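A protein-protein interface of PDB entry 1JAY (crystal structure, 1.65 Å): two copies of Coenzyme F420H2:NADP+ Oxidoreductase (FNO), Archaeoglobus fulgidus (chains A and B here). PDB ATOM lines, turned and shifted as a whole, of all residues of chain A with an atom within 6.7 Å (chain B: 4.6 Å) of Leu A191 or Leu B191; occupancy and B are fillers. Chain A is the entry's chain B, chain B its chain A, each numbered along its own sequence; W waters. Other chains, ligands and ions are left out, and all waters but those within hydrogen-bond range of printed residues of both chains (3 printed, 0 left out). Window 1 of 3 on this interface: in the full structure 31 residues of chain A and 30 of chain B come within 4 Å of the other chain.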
ATOM      1  N   VAL A  98     -18.988 -20.443 -31.568  1.00  0.00           N
ATOM      2  CA  VAL A  98     -18.063 -20.967 -30.575  1.00  0.00           C
ATOM      3  C   VAL A  98     -16.764 -20.149 -30.491  1.00  0.00           C
ATOM      4  O   VAL A  98     -16.022 -20.060 -31.465  1.00  0.00           O
ATOM      5  CB  VAL A  98     -17.633 -22.404 -30.897  1.00  0.00           C
ATOM      6  CG1 VAL A  98     -16.689 -22.901 -29.784  1.00  0.00           C
ATOM      7  CG2 VAL A  98     -18.865 -23.322 -31.087  1.00  0.00           C
ATOM      8  N   TYR A 109     -11.081 -22.118 -24.947  1.00  0.00           N
ATOM      9  CA  TYR A 109     -12.297 -21.305 -25.047  1.00  0.00           C
ATOM     10  C   TYR A 109     -11.755 -19.877 -25.017  1.00  0.00           C
ATOM     11  O   TYR A 109     -11.016 -19.513 -24.098  1.00  0.00           O
ATOM     12  CB  TYR A 109     -13.202 -21.579 -23.840  1.00  0.00           C
ATOM     13  CG  TYR A 109     -14.541 -20.906 -23.948  1.00  0.00           C
ATOM     14  CD1 TYR A 109     -15.538 -21.443 -24.758  1.00  0.00           C
ATOM     15  CD2 TYR A 109     -14.808 -19.707 -23.260  1.00  0.00           C
ATOM     16  CE1 TYR A 109     -16.782 -20.813 -24.897  1.00  0.00           C
ATOM     17  CE2 TYR A 109     -16.049 -19.069 -23.390  1.00  0.00           C
ATOM     18  CZ  TYR A 109     -17.031 -19.632 -24.212  1.00  0.00           C
ATOM     19  OH  TYR A 109     -18.281 -19.024 -24.340  1.00  0.00           O
ATOM     20  N   HIS A 133     -23.692 -26.137 -31.534  1.00  0.00           N
ATOM     21  CA  HIS A 133     -22.243 -26.093 -31.387  1.00  0.00           C
ATOM     22  C   HIS A 133     -21.483 -27.370 -31.578  1.00  0.00           C
ATOM     23  O   HIS A 133     -20.323 -27.334 -31.983  1.00  0.00           O
ATOM     24  CB  HIS A 133     -21.874 -25.567 -30.000  1.00  0.00           C
ATOM     25  CG  HIS A 133     -22.737 -24.433 -29.567  1.00  0.00           C
ATOM     26  ND1 HIS A 133     -23.969 -24.633 -28.982  1.00  0.00           N
ATOM     27  CD2 HIS A 133     -22.572 -23.090 -29.658  1.00  0.00           C
ATOM     28  CE1 HIS A 133     -24.522 -23.463 -28.722  1.00  0.00           C
ATOM     29  NE2 HIS A 133     -23.700 -22.512 -29.126  1.00  0.00           N
ATOM     30  N   THR A 134     -22.117 -28.500 -31.298  1.00  0.00           N
ATOM     31  CA  THR A 134     -21.388 -29.753 -31.357  1.00  0.00           C
ATOM     32  C   THR A 134     -21.771 -30.650 -32.518  1.00  0.00           C
ATOM     33  O   THR A 134     -21.684 -31.864 -32.407  1.00  0.00           O
ATOM     34  CB  THR A 134     -21.566 -30.549 -30.030  1.00  0.00           C
ATOM     35  OG1 THR A 134     -22.953 -30.860 -29.835  1.00  0.00           O
ATOM     36  CG2 THR A 134     -21.037 -29.700 -28.822  1.00  0.00           C
ATOM     37  N   PRO A 152     -27.519 -29.608 -27.112  1.00  0.00           N
ATOM     38  CA  PRO A 152     -27.951 -28.793 -25.976  1.00  0.00           C
ATOM     39  C   PRO A 152     -28.447 -27.435 -26.508  1.00  0.00           C
ATOM     40  O   PRO A 152     -27.834 -26.838 -27.391  1.00  0.00           O
ATOM     41  CB  PRO A 152     -26.673 -28.642 -25.144  1.00  0.00           C
ATOM     42  CG  PRO A 152     -25.887 -29.889 -25.465  1.00  0.00           C
ATOM     43  CD  PRO A 152     -26.113 -30.023 -26.980  1.00  0.00           C
ATOM     44  N   ARG A 186     -22.141 -20.633 -21.973  1.00  0.00           N
ATOM     45  CA  ARG A 186     -20.701 -20.843 -21.954  1.00  0.00           C
ATOM     46  C   ARG A 186     -20.358 -22.329 -21.750  1.00  0.00           C
ATOM     47  O   ARG A 186     -19.391 -22.846 -22.305  1.00  0.00           O
ATOM     48  CB  ARG A 186     -20.073 -19.999 -20.847  1.00  0.00           C
ATOM     49  CG  ARG A 186     -18.558 -19.976 -20.853  1.00  0.00           C
ATOM     50  CD  ARG A 186     -18.119 -19.084 -19.684  1.00  0.00           C
ATOM     51  NE  ARG A 186     -16.697 -18.753 -19.642  1.00  0.00           N
ATOM     52  CZ  ARG A 186     -15.719 -19.626 -19.832  1.00  0.00           C
ATOM     53  NH1 ARG A 186     -16.003 -20.886 -20.102  1.00  0.00           N
ATOM     54  NH2 ARG A 186     -14.453 -19.244 -19.694  1.00  0.00           N
ATOM     55  N   LEU A 187     -21.148 -23.023 -20.941  1.00  0.00           N
ATOM     56  CA  LEU A 187     -20.897 -24.451 -20.697  1.00  0.00           C
ATOM     57  C   LEU A 187     -21.174 -25.272 -21.953  1.00  0.00           C
ATOM     58  O   LEU A 187     -20.527 -26.297 -22.175  1.00  0.00           O
ATOM     59  CB  LEU A 187     -21.806 -24.978 -19.566  1.00  0.00           C
ATOM     60  CG  LEU A 187     -21.473 -24.408 -18.185  1.00  0.00           C
ATOM     61  CD1 LEU A 187     -22.556 -24.864 -17.186  1.00  0.00           C
ATOM     62  CD2 LEU A 187     -20.094 -24.882 -17.745  1.00  0.00           C
ATOM     63  N   VAL A 188     -22.154 -24.841 -22.753  1.00  0.00           N
ATOM     64  CA  VAL A 188     -22.481 -25.572 -23.980  1.00  0.00           C
ATOM     65  C   VAL A 188     -21.415 -25.295 -25.053  1.00  0.00           C
ATOM     66  O   VAL A 188     -20.936 -26.210 -25.729  1.00  0.00           O
ATOM     67  CB  VAL A 188     -23.864 -25.153 -24.525  1.00  0.00           C
ATOM     68  CG1 VAL A 188     -24.135 -25.868 -25.856  1.00  0.00           C
ATOM     69  CG2 VAL A 188     -24.967 -25.533 -23.509  1.00  0.00           C
ATOM     70  N   GLU A 189     -21.079 -24.019 -25.210  1.00  0.00           N
ATOM     71  CA  GLU A 189     -20.068 -23.579 -26.177  1.00  0.00           C
ATOM     72  C   GLU A 189     -18.713 -24.223 -25.886  1.00  0.00           C
ATOM     73  O   GLU A 189     -17.960 -24.536 -26.802  1.00  0.00           O
ATOM     74  CB  GLU A 189     -19.941 -22.056 -26.131  1.00  0.00           C
ATOM     75  CG  GLU A 189     -21.174 -21.337 -26.705  1.00  0.00           C
ATOM     76  CD  GLU A 189     -21.129 -19.818 -26.489  1.00  0.00           C
ATOM     77  OE1 GLU A 189     -20.028 -19.273 -26.189  1.00  0.00           O
ATOM     78  OE2 GLU A 189     -22.192 -19.178 -26.631  1.00  0.00           O
ATOM     79  N   SER A 190     -18.423 -24.444 -24.612  1.00  0.00           N
ATOM     80  CA  SER A 190     -17.156 -25.057 -24.214  1.00  0.00           C
ATOM     81  C   SER A 190     -17.006 -26.510 -24.636  1.00  0.00           C
ATOM     82  O   SER A 190     -15.902 -27.042 -24.643  1.00  0.00           O
ATOM     83  CB  SER A 190     -16.963 -24.944 -22.689  1.00  0.00           C
ATOM     84  OG  SER A 190     -16.802 -23.561 -22.383  1.00  0.00           O
ATOM     85  N   LEU A 191     -18.108 -27.157 -24.984  1.00  0.00           N
ATOM     86  CA  LEU A 191     -18.024 -28.543 -25.424  1.00  0.00           C
ATOM     87  C   LEU A 191     -17.192 -28.631 -26.702  1.00  0.00           C
ATOM     88  O   LEU A 191     -16.516 -29.629 -26.941  1.00  0.00           O
ATOM     89  CB  LEU A 191     -19.424 -29.093 -25.744  1.00  0.00           C
ATOM     90  CG  LEU A 191     -20.406 -29.297 -24.602  1.00  0.00           C
ATOM     91  CD1 LEU A 191     -21.766 -29.657 -25.237  1.00  0.00           C
ATOM     92  CD2 LEU A 191     -19.936 -30.437 -23.652  1.00  0.00           C
ATOM     93  N   THR A 192     -17.246 -27.594 -27.528  1.00  0.00           N
ATOM     94  CA  THR A 192     -16.534 -27.669 -28.808  1.00  0.00           C
ATOM     95  C   THR A 192     -15.021 -27.723 -28.651  1.00  0.00           C
ATOM     96  O   THR A 192     -14.379 -28.607 -29.227  1.00  0.00           O
ATOM     97  CB  THR A 192     -16.987 -26.539 -29.741  1.00  0.00           C
ATOM     98  OG1 THR A 192     -18.383 -26.686 -29.972  1.00  0.00           O
ATOM     99  CG2 THR A 192     -16.269 -26.615 -31.084  1.00  0.00           C
ATOM    100  N   PRO A 193     -14.420 -26.770 -27.905  1.00  0.00           N
ATOM    101  CA  PRO A 193     -12.968 -26.878 -27.762  1.00  0.00           C
ATOM    102  C   PRO A 193     -12.604 -28.218 -27.073  1.00  0.00           C
ATOM    103  O   PRO A 193     -11.536 -28.762 -27.333  1.00  0.00           O
ATOM    104  CB  PRO A 193     -12.580 -25.640 -26.928  1.00  0.00           C
ATOM    105  CG  PRO A 193     -13.897 -25.102 -26.408  1.00  0.00           C
ATOM    106  CD  PRO A 193     -14.906 -25.459 -27.442  1.00  0.00           C
ATOM    107  N   LEU A 194     -13.462 -28.736 -26.190  1.00  0.00           N
ATOM    108  CA  LEU A 194     -13.147 -30.039 -25.561  1.00  0.00           C
ATOM    109  C   LEU A 194     -13.111 -31.130 -26.645  1.00  0.00           C
ATOM    110  O   LEU A 194     -12.186 -31.931 -26.697  1.00  0.00           O
ATOM    111  CB  LEU A 194     -14.183 -30.400 -24.473  1.00  0.00           C
ATOM    112  CG  LEU A 194     -14.036 -31.828 -23.896  1.00  0.00           C
ATOM    113  CD1 LEU A 194     -12.686 -32.000 -23.209  1.00  0.00           C
ATOM    114  CD2 LEU A 194     -15.141 -32.093 -22.927  1.00  0.00           C
ATOM    115  N   ILE A 195     -14.107 -31.130 -27.525  1.00  0.00           N
ATOM    116  CA  ILE A 195     -14.169 -32.120 -28.600  1.00  0.00           C
ATOM    117  C   ILE A 195     -12.957 -31.988 -29.535  1.00  0.00           C
ATOM    118  O   ILE A 195     -12.327 -32.983 -29.917  1.00  0.00           O
ATOM    119  CB  ILE A 195     -15.503 -31.969 -29.406  1.00  0.00           C
ATOM    120  CG1 ILE A 195     -16.680 -32.464 -28.551  1.00  0.00           C
ATOM    121  CG2 ILE A 195     -15.459 -32.827 -30.689  1.00  0.00           C
ATOM    122  CD1 ILE A 195     -18.068 -32.127 -29.158  1.00  0.00           C
ATOM    123  N   LEU A 196     -12.630 -30.761 -29.919  1.00  0.00           N
ATOM    124  CA  LEU A 196     -11.486 -30.566 -30.804  1.00  0.00           C
ATOM    125  C   LEU A 196     -10.205 -31.098 -30.150  1.00  0.00           C
ATOM    126  O   LEU A 196      -9.333 -31.663 -30.820  1.00  0.00           O
ATOM    127  CB  LEU A 196     -11.357 -29.088 -31.164  1.00  0.00           C
ATOM    128  CG  LEU A 196     -12.531 -28.547 -31.983  1.00  0.00           C
ATOM    129  CD1 LEU A 196     -12.402 -27.033 -32.169  1.00  0.00           C
ATOM    130  CD2 LEU A 196     -12.554 -29.275 -33.359  1.00  0.00           C
ATOM    131  N   ILE A 198     -10.039 -33.596 -27.961  1.00  0.00           N
ATOM    132  CA  ILE A 198     -10.100 -35.058 -28.000  1.00  0.00           C
ATOM    133  C   ILE A 198      -9.737 -35.576 -29.399  1.00  0.00           C
ATOM    134  O   ILE A 198      -9.002 -36.554 -29.536  1.00  0.00           O
ATOM    135  CB  ILE A 198     -11.477 -35.535 -27.570  1.00  0.00           C
ATOM    136  CG1 ILE A 198     -11.565 -35.388 -26.038  1.00  0.00           C
ATOM    137  CG2 ILE A 198     -11.712 -37.019 -27.990  1.00  0.00           C
ATOM    138  CD1 ILE A 198     -12.957 -35.619 -25.490  1.00  0.00           C
ATOM    139  N   ILE A 209     -21.726 -35.444 -29.613  1.00  0.00           N
ATOM    140  CA  ILE A 209     -21.879 -35.977 -28.262  1.00  0.00           C
ATOM    141  C   ILE A 209     -23.257 -36.540 -27.993  1.00  0.00           C
ATOM    142  O   ILE A 209     -24.240 -36.189 -28.666  1.00  0.00           O
ATOM    143  CB  ILE A 209     -21.572 -34.897 -27.199  1.00  0.00           C
ATOM    144  CG1 ILE A 209     -22.284 -33.590 -27.536  1.00  0.00           C
ATOM    145  CG2 ILE A 209     -20.082 -34.608 -27.199  1.00  0.00           C
ATOM    146  CD1 ILE A 209     -23.466 -33.284 -26.723  1.00  0.00           C
ATOM    147  N   PHE A 211     -25.685 -37.820 -24.453  1.00  0.00           N
ATOM    148  CA  PHE A 211     -25.798 -37.921 -23.003  1.00  0.00           C
ATOM    149  C   PHE A 211     -26.592 -39.188 -22.761  1.00  0.00           C
ATOM    150  O   PHE A 211     -27.719 -39.323 -23.256  1.00  0.00           O
ATOM    151  CB  PHE A 211     -26.520 -36.714 -22.433  1.00  0.00           C
ATOM    152  CG  PHE A 211     -25.805 -35.430 -22.696  1.00  0.00           C
ATOM    153  CD1 PHE A 211     -26.115 -34.651 -23.810  1.00  0.00           C
ATOM    154  CD2 PHE A 211     -24.781 -35.018 -21.853  1.00  0.00           C
ATOM    155  CE1 PHE A 211     -25.403 -33.482 -24.066  1.00  0.00           C
ATOM    156  CE2 PHE A 211     -24.072 -33.860 -22.100  1.00  0.00           C
ATOM    157  CZ  PHE A 211     -24.385 -33.087 -23.210  1.00  0.00           C
ATOM    158  N   THR B 134     -17.193 -37.234 -15.198  1.00  0.00           N
ATOM    159  CA  THR B 134     -18.533 -37.436 -15.744  1.00  0.00           C
ATOM    160  C   THR B 134     -19.112 -38.824 -15.502  1.00  0.00           C
ATOM    161  O   THR B 134     -19.977 -39.271 -16.238  1.00  0.00           O
ATOM    162  CB  THR B 134     -18.547 -37.122 -17.265  1.00  0.00           C
ATOM    163  OG1 THR B 134     -17.676 -38.020 -17.963  1.00  0.00           O
ATOM    164  CG2 THR B 134     -18.045 -35.666 -17.518  1.00  0.00           C
ATOM    165  N   PRO B 152     -12.906 -38.402 -20.489  1.00  0.00           N
ATOM    166  CA  PRO B 152     -11.817 -37.547 -20.977  1.00  0.00           C
ATOM    167  C   PRO B 152     -10.747 -37.545 -19.891  1.00  0.00           C
ATOM    168  O   PRO B 152     -11.064 -37.429 -18.697  1.00  0.00           O
ATOM    169  CB  PRO B 152     -12.468 -36.153 -21.095  1.00  0.00           C
ATOM    170  CG  PRO B 152     -13.920 -36.472 -21.340  1.00  0.00           C
ATOM    171  CD  PRO B 152     -14.169 -37.651 -20.390  1.00  0.00           C
ATOM    172  N   LEU B 187     -11.863 -27.525 -19.274  1.00  0.00           N
ATOM    173  CA  LEU B 187     -12.867 -27.947 -20.253  1.00  0.00           C
ATOM    174  C   LEU B 187     -13.491 -29.295 -19.850  1.00  0.00           C
ATOM    175  O   LEU B 187     -14.676 -29.523 -20.058  1.00  0.00           O
ATOM    176  CB  LEU B 187     -12.237 -28.086 -21.652  1.00  0.00           C
ATOM    177  CG  LEU B 187     -11.719 -26.777 -22.287  1.00  0.00           C
ATOM    178  CD1 LEU B 187     -10.935 -27.129 -23.584  1.00  0.00           C
ATOM    179  CD2 LEU B 187     -12.906 -25.810 -22.593  1.00  0.00           C
ATOM    180  N   VAL B 188     -12.683 -30.192 -19.301  1.00  0.00           N
ATOM    181  CA  VAL B 188     -13.209 -31.500 -18.888  1.00  0.00           C
ATOM    182  C   VAL B 188     -14.090 -31.381 -17.644  1.00  0.00           C
ATOM    183  O   VAL B 188     -15.182 -31.934 -17.591  1.00  0.00           O
ATOM    184  CB  VAL B 188     -12.061 -32.482 -18.589  1.00  0.00           C
ATOM    185  CG1 VAL B 188     -12.624 -33.824 -18.128  1.00  0.00           C
ATOM    186  CG2 VAL B 188     -11.178 -32.639 -19.856  1.00  0.00           C
ATOM    187  N   GLU B 189     -13.603 -30.662 -16.634  1.00  0.00           N
ATOM    188  CA  GLU B 189     -14.366 -30.478 -15.397  1.00  0.00           C
ATOM    189  C   GLU B 189     -15.682 -29.767 -15.649  1.00  0.00           C
ATOM    190  O   GLU B 189     -16.676 -30.030 -14.956  1.00  0.00           O
ATOM    191  CB  GLU B 189     -13.536 -29.673 -14.376  1.00  0.00           C
ATOM    192  CG  GLU B 189     -12.293 -30.413 -13.870  1.00  0.00           C
ATOM    193  CD  GLU B 189     -11.355 -29.519 -13.047  1.00  0.00           C
ATOM    194  OE1 GLU B 189     -11.786 -28.444 -12.567  1.00  0.00           O
ATOM    195  OE2 GLU B 189     -10.172 -29.913 -12.884  1.00  0.00           O
ATOM    196  N   SER B 190     -15.691 -28.865 -16.633  1.00  0.00           N
ATOM    197  CA  SER B 190     -16.902 -28.118 -16.967  1.00  0.00           C
ATOM    198  C   SER B 190     -18.003 -29.002 -17.541  1.00  0.00           C
ATOM    199  O   SER B 190     -19.160 -28.579 -17.593  1.00  0.00           O
ATOM    200  CB  SER B 190     -16.598 -26.968 -17.952  1.00  0.00           C
ATOM    201  OG  SER B 190     -15.791 -26.005 -17.300  1.00  0.00           O
ATOM    202  N   LEU B 191     -17.658 -30.215 -17.958  1.00  0.00           N
ATOM    203  CA  LEU B 191     -18.678 -31.118 -18.477  1.00  0.00           C
ATOM    204  C   LEU B 191     -19.693 -31.451 -17.409  1.00  0.00           C
ATOM    205  O   LEU B 191     -20.864 -31.650 -17.712  1.00  0.00           O
ATOM    206  CB  LEU B 191     -18.079 -32.444 -18.934  1.00  0.00           C
ATOM    207  CG  LEU B 191     -17.218 -32.395 -20.184  1.00  0.00           C
ATOM    208  CD1 LEU B 191     -16.578 -33.770 -20.409  1.00  0.00           C
ATOM    209  CD2 LEU B 191     -18.076 -31.973 -21.370  1.00  0.00           C
ATOM    210  N   THR B 192     -19.258 -31.510 -16.155  1.00  0.00           N
ATOM    211  CA  THR B 192     -20.176 -31.893 -15.085  1.00  0.00           C
ATOM    212  C   THR B 192     -21.312 -30.899 -14.843  1.00  0.00           C
ATOM    213  O   THR B 192     -22.497 -31.298 -14.808  1.00  0.00           O
ATOM    214  CB  THR B 192     -19.362 -32.241 -13.809  1.00  0.00           C
ATOM    215  OG1 THR B 192     -18.457 -33.304 -14.126  1.00  0.00           O
ATOM    216  CG2 THR B 192     -20.260 -32.694 -12.687  1.00  0.00           C
ATOM    217  N   PRO B 193     -21.002 -29.595 -14.684  1.00  0.00           N
ATOM    218  CA  PRO B 193     -22.142 -28.702 -14.474  1.00  0.00           C
ATOM    219  C   PRO B 193     -23.044 -28.694 -15.723  1.00  0.00           C
ATOM    220  O   PRO B 193     -24.250 -28.496 -15.614  1.00  0.00           O
ATOM    221  CB  PRO B 193     -21.505 -27.332 -14.195  1.00  0.00           C
ATOM    222  CG  PRO B 193     -20.036 -27.491 -14.513  1.00  0.00           C
ATOM    223  CD  PRO B 193     -19.723 -28.946 -14.362  1.00  0.00           C
ATOM    224  N   LEU B 194     -22.471 -28.921 -16.909  1.00  0.00           N
ATOM    225  CA  LEU B 194     -23.316 -28.971 -18.107  1.00  0.00           C
ATOM    226  C   LEU B 194     -24.269 -30.175 -17.990  1.00  0.00           C
ATOM    227  O   LEU B 194     -25.495 -30.057 -18.208  1.00  0.00           O
ATOM    228  CB  LEU B 194     -22.480 -29.085 -19.384  1.00  0.00           C
ATOM    229  CG  LEU B 194     -23.362 -29.296 -20.630  1.00  0.00           C
ATOM    230  CD1 LEU B 194     -24.336 -28.164 -20.753  1.00  0.00           C
ATOM    231  CD2 LEU B 194     -22.527 -29.388 -21.850  1.00  0.00           C
ATOM    232  N   ILE B 195     -23.724 -31.327 -17.609  1.00  0.00           N
ATOM    233  CA  ILE B 195     -24.560 -32.516 -17.449  1.00  0.00           C
ATOM    234  C   ILE B 195     -25.634 -32.306 -16.378  1.00  0.00           C
ATOM    235  O   ILE B 195     -26.793 -32.678 -16.580  1.00  0.00           O
ATOM    236  CB  ILE B 195     -23.702 -33.747 -17.098  1.00  0.00           C
ATOM    237  CG1 ILE B 195     -22.883 -34.150 -18.325  1.00  0.00           C
ATOM    238  CG2 ILE B 195     -24.599 -34.922 -16.626  1.00  0.00           C
ATOM    239  CD1 ILE B 195     -21.799 -35.193 -18.024  1.00  0.00           C
ATOM    240  N   ILE B 209     -21.457 -39.260 -20.596  1.00  0.00           N
ATOM    241  CA  ILE B 209     -21.413 -38.769 -21.965  1.00  0.00           C
ATOM    242  C   ILE B 209     -20.604 -39.686 -22.871  1.00  0.00           C
ATOM    243  O   ILE B 209     -19.742 -40.439 -22.407  1.00  0.00           O
ATOM    244  CB  ILE B 209     -20.809 -37.358 -22.033  1.00  0.00           C
ATOM    245  CG1 ILE B 209     -19.385 -37.369 -21.477  1.00  0.00           C
ATOM    246  CG2 ILE B 209     -21.683 -36.393 -21.245  1.00  0.00           C
ATOM    247  CD1 ILE B 209     -18.663 -36.051 -21.640  1.00  0.00           C
HETATM  248  O   HOH W   1     -16.446 -28.329 -21.885  1.00  0.00           O
HETATM  249  O   HOH W   2     -18.963 -28.007 -20.585  1.00  0.00           O
HETATM  250  O   HOH W   3     -15.978 -23.454 -17.973  1.00  0.00           O
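The backbone carbonyl oxygen of Arg A186 is in hydrogen-bond range of the side-chain hydroxyl of Ser A190, at 2.7 Å.
Leu A191 touches two residues of chain B.
Leu B191 touches just these residues of chain A: Leu A191 (3.3 Å) and Leu A194 (3.3 Å).
Of the printed residues of chain A, Val B188 touches Leu A194 (3.7 Å).
Of the printed residues of chain B, Phe A211 touches Ile B195 (3.97 Å) and Ile B209 (3.4 Å).
Of the printed residues of chain B, Leu A187 touches Ser B190 and Leu B194.
Glu A189 touches none of the printed residues of chain B.
Pro A193 touches none of the printed residues of chain B.
The nearest printed residue of chain A that does not touch Leu B191 is Leu A187 (5.9 Å).
Of the 19 printed residues of chain A, 6 touch a printed residue of chain B.
Printed residues of chain A that touch a printed residue of chain B: Leu A187, Val A188, Ser A190, Leu A191, Leu A194 and Phe A211.
Of the 12 printed residues of chain B, 7 touch a printed residue of chain A.
Printed residues of chain B that touch a printed residue of chain A: Leu B187, Val B188, Ser B190, Leu B191, Leu B194, Ile B195 and Ile B209.
Hydrophobic or aromatic side chains of chain B that line the printed part of chain A: Leu B187, Val B188, Leu B191, Leu B194, Ile B195 and Ile B209.
Among the printed residues, 11 pairs touch across the chains.
Ser B190 touches Leu A187.
O of Leu A187 touches CD2 of Leu B194, at 3.7 Å.
Leu B194 touches Val A188.
Ser A190 touches Leu B187 (O to CD2, 3.8 Å).
Leu A191 touches Leu B191 (CD2 to CD2, 3.3 Å).
CD2 of Leu B194 touches CD2 of Leu A191, 3.3 Å away.
Leu A194 touches Val B188 (CD1 to CG2, 3.7 Å).
Leu A194 touches Leu B191.
Phe A211 touches Ile B195.
Ile B209 touches Phe A211.
Water W3 bridges the side-chain hydroxyl of Ser B190 and the guanidinium group of Arg A186.
Water W1 bridges O of Leu B187 (2.8 Å) and O of Ser A190 (3.1 Å).
Water W2 bridges O of Leu A187 (2.8 Å) and O of Ser B190 (3.1 Å).
Leu A187 touches Ser B190, and with the chains exchanged Ser A190 touches Leu B187.
Leu A187 touches Leu B194, and with the chains exchanged Leu A194 touches Leu B187.
Val A188 touches Leu B194, and with the chains exchanged Leu A194 touches Val B188.
Leu B191 touches its own counterpart, Leu A191.
Positions printed for both chains: 134, 152, 187, 188, 189, 190, 191, 192, 193, 194, 195 and 209.
Of the 11 pairs that touch across the chains among the printed residues, 9 have their exchanged pair printed and touching as well.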
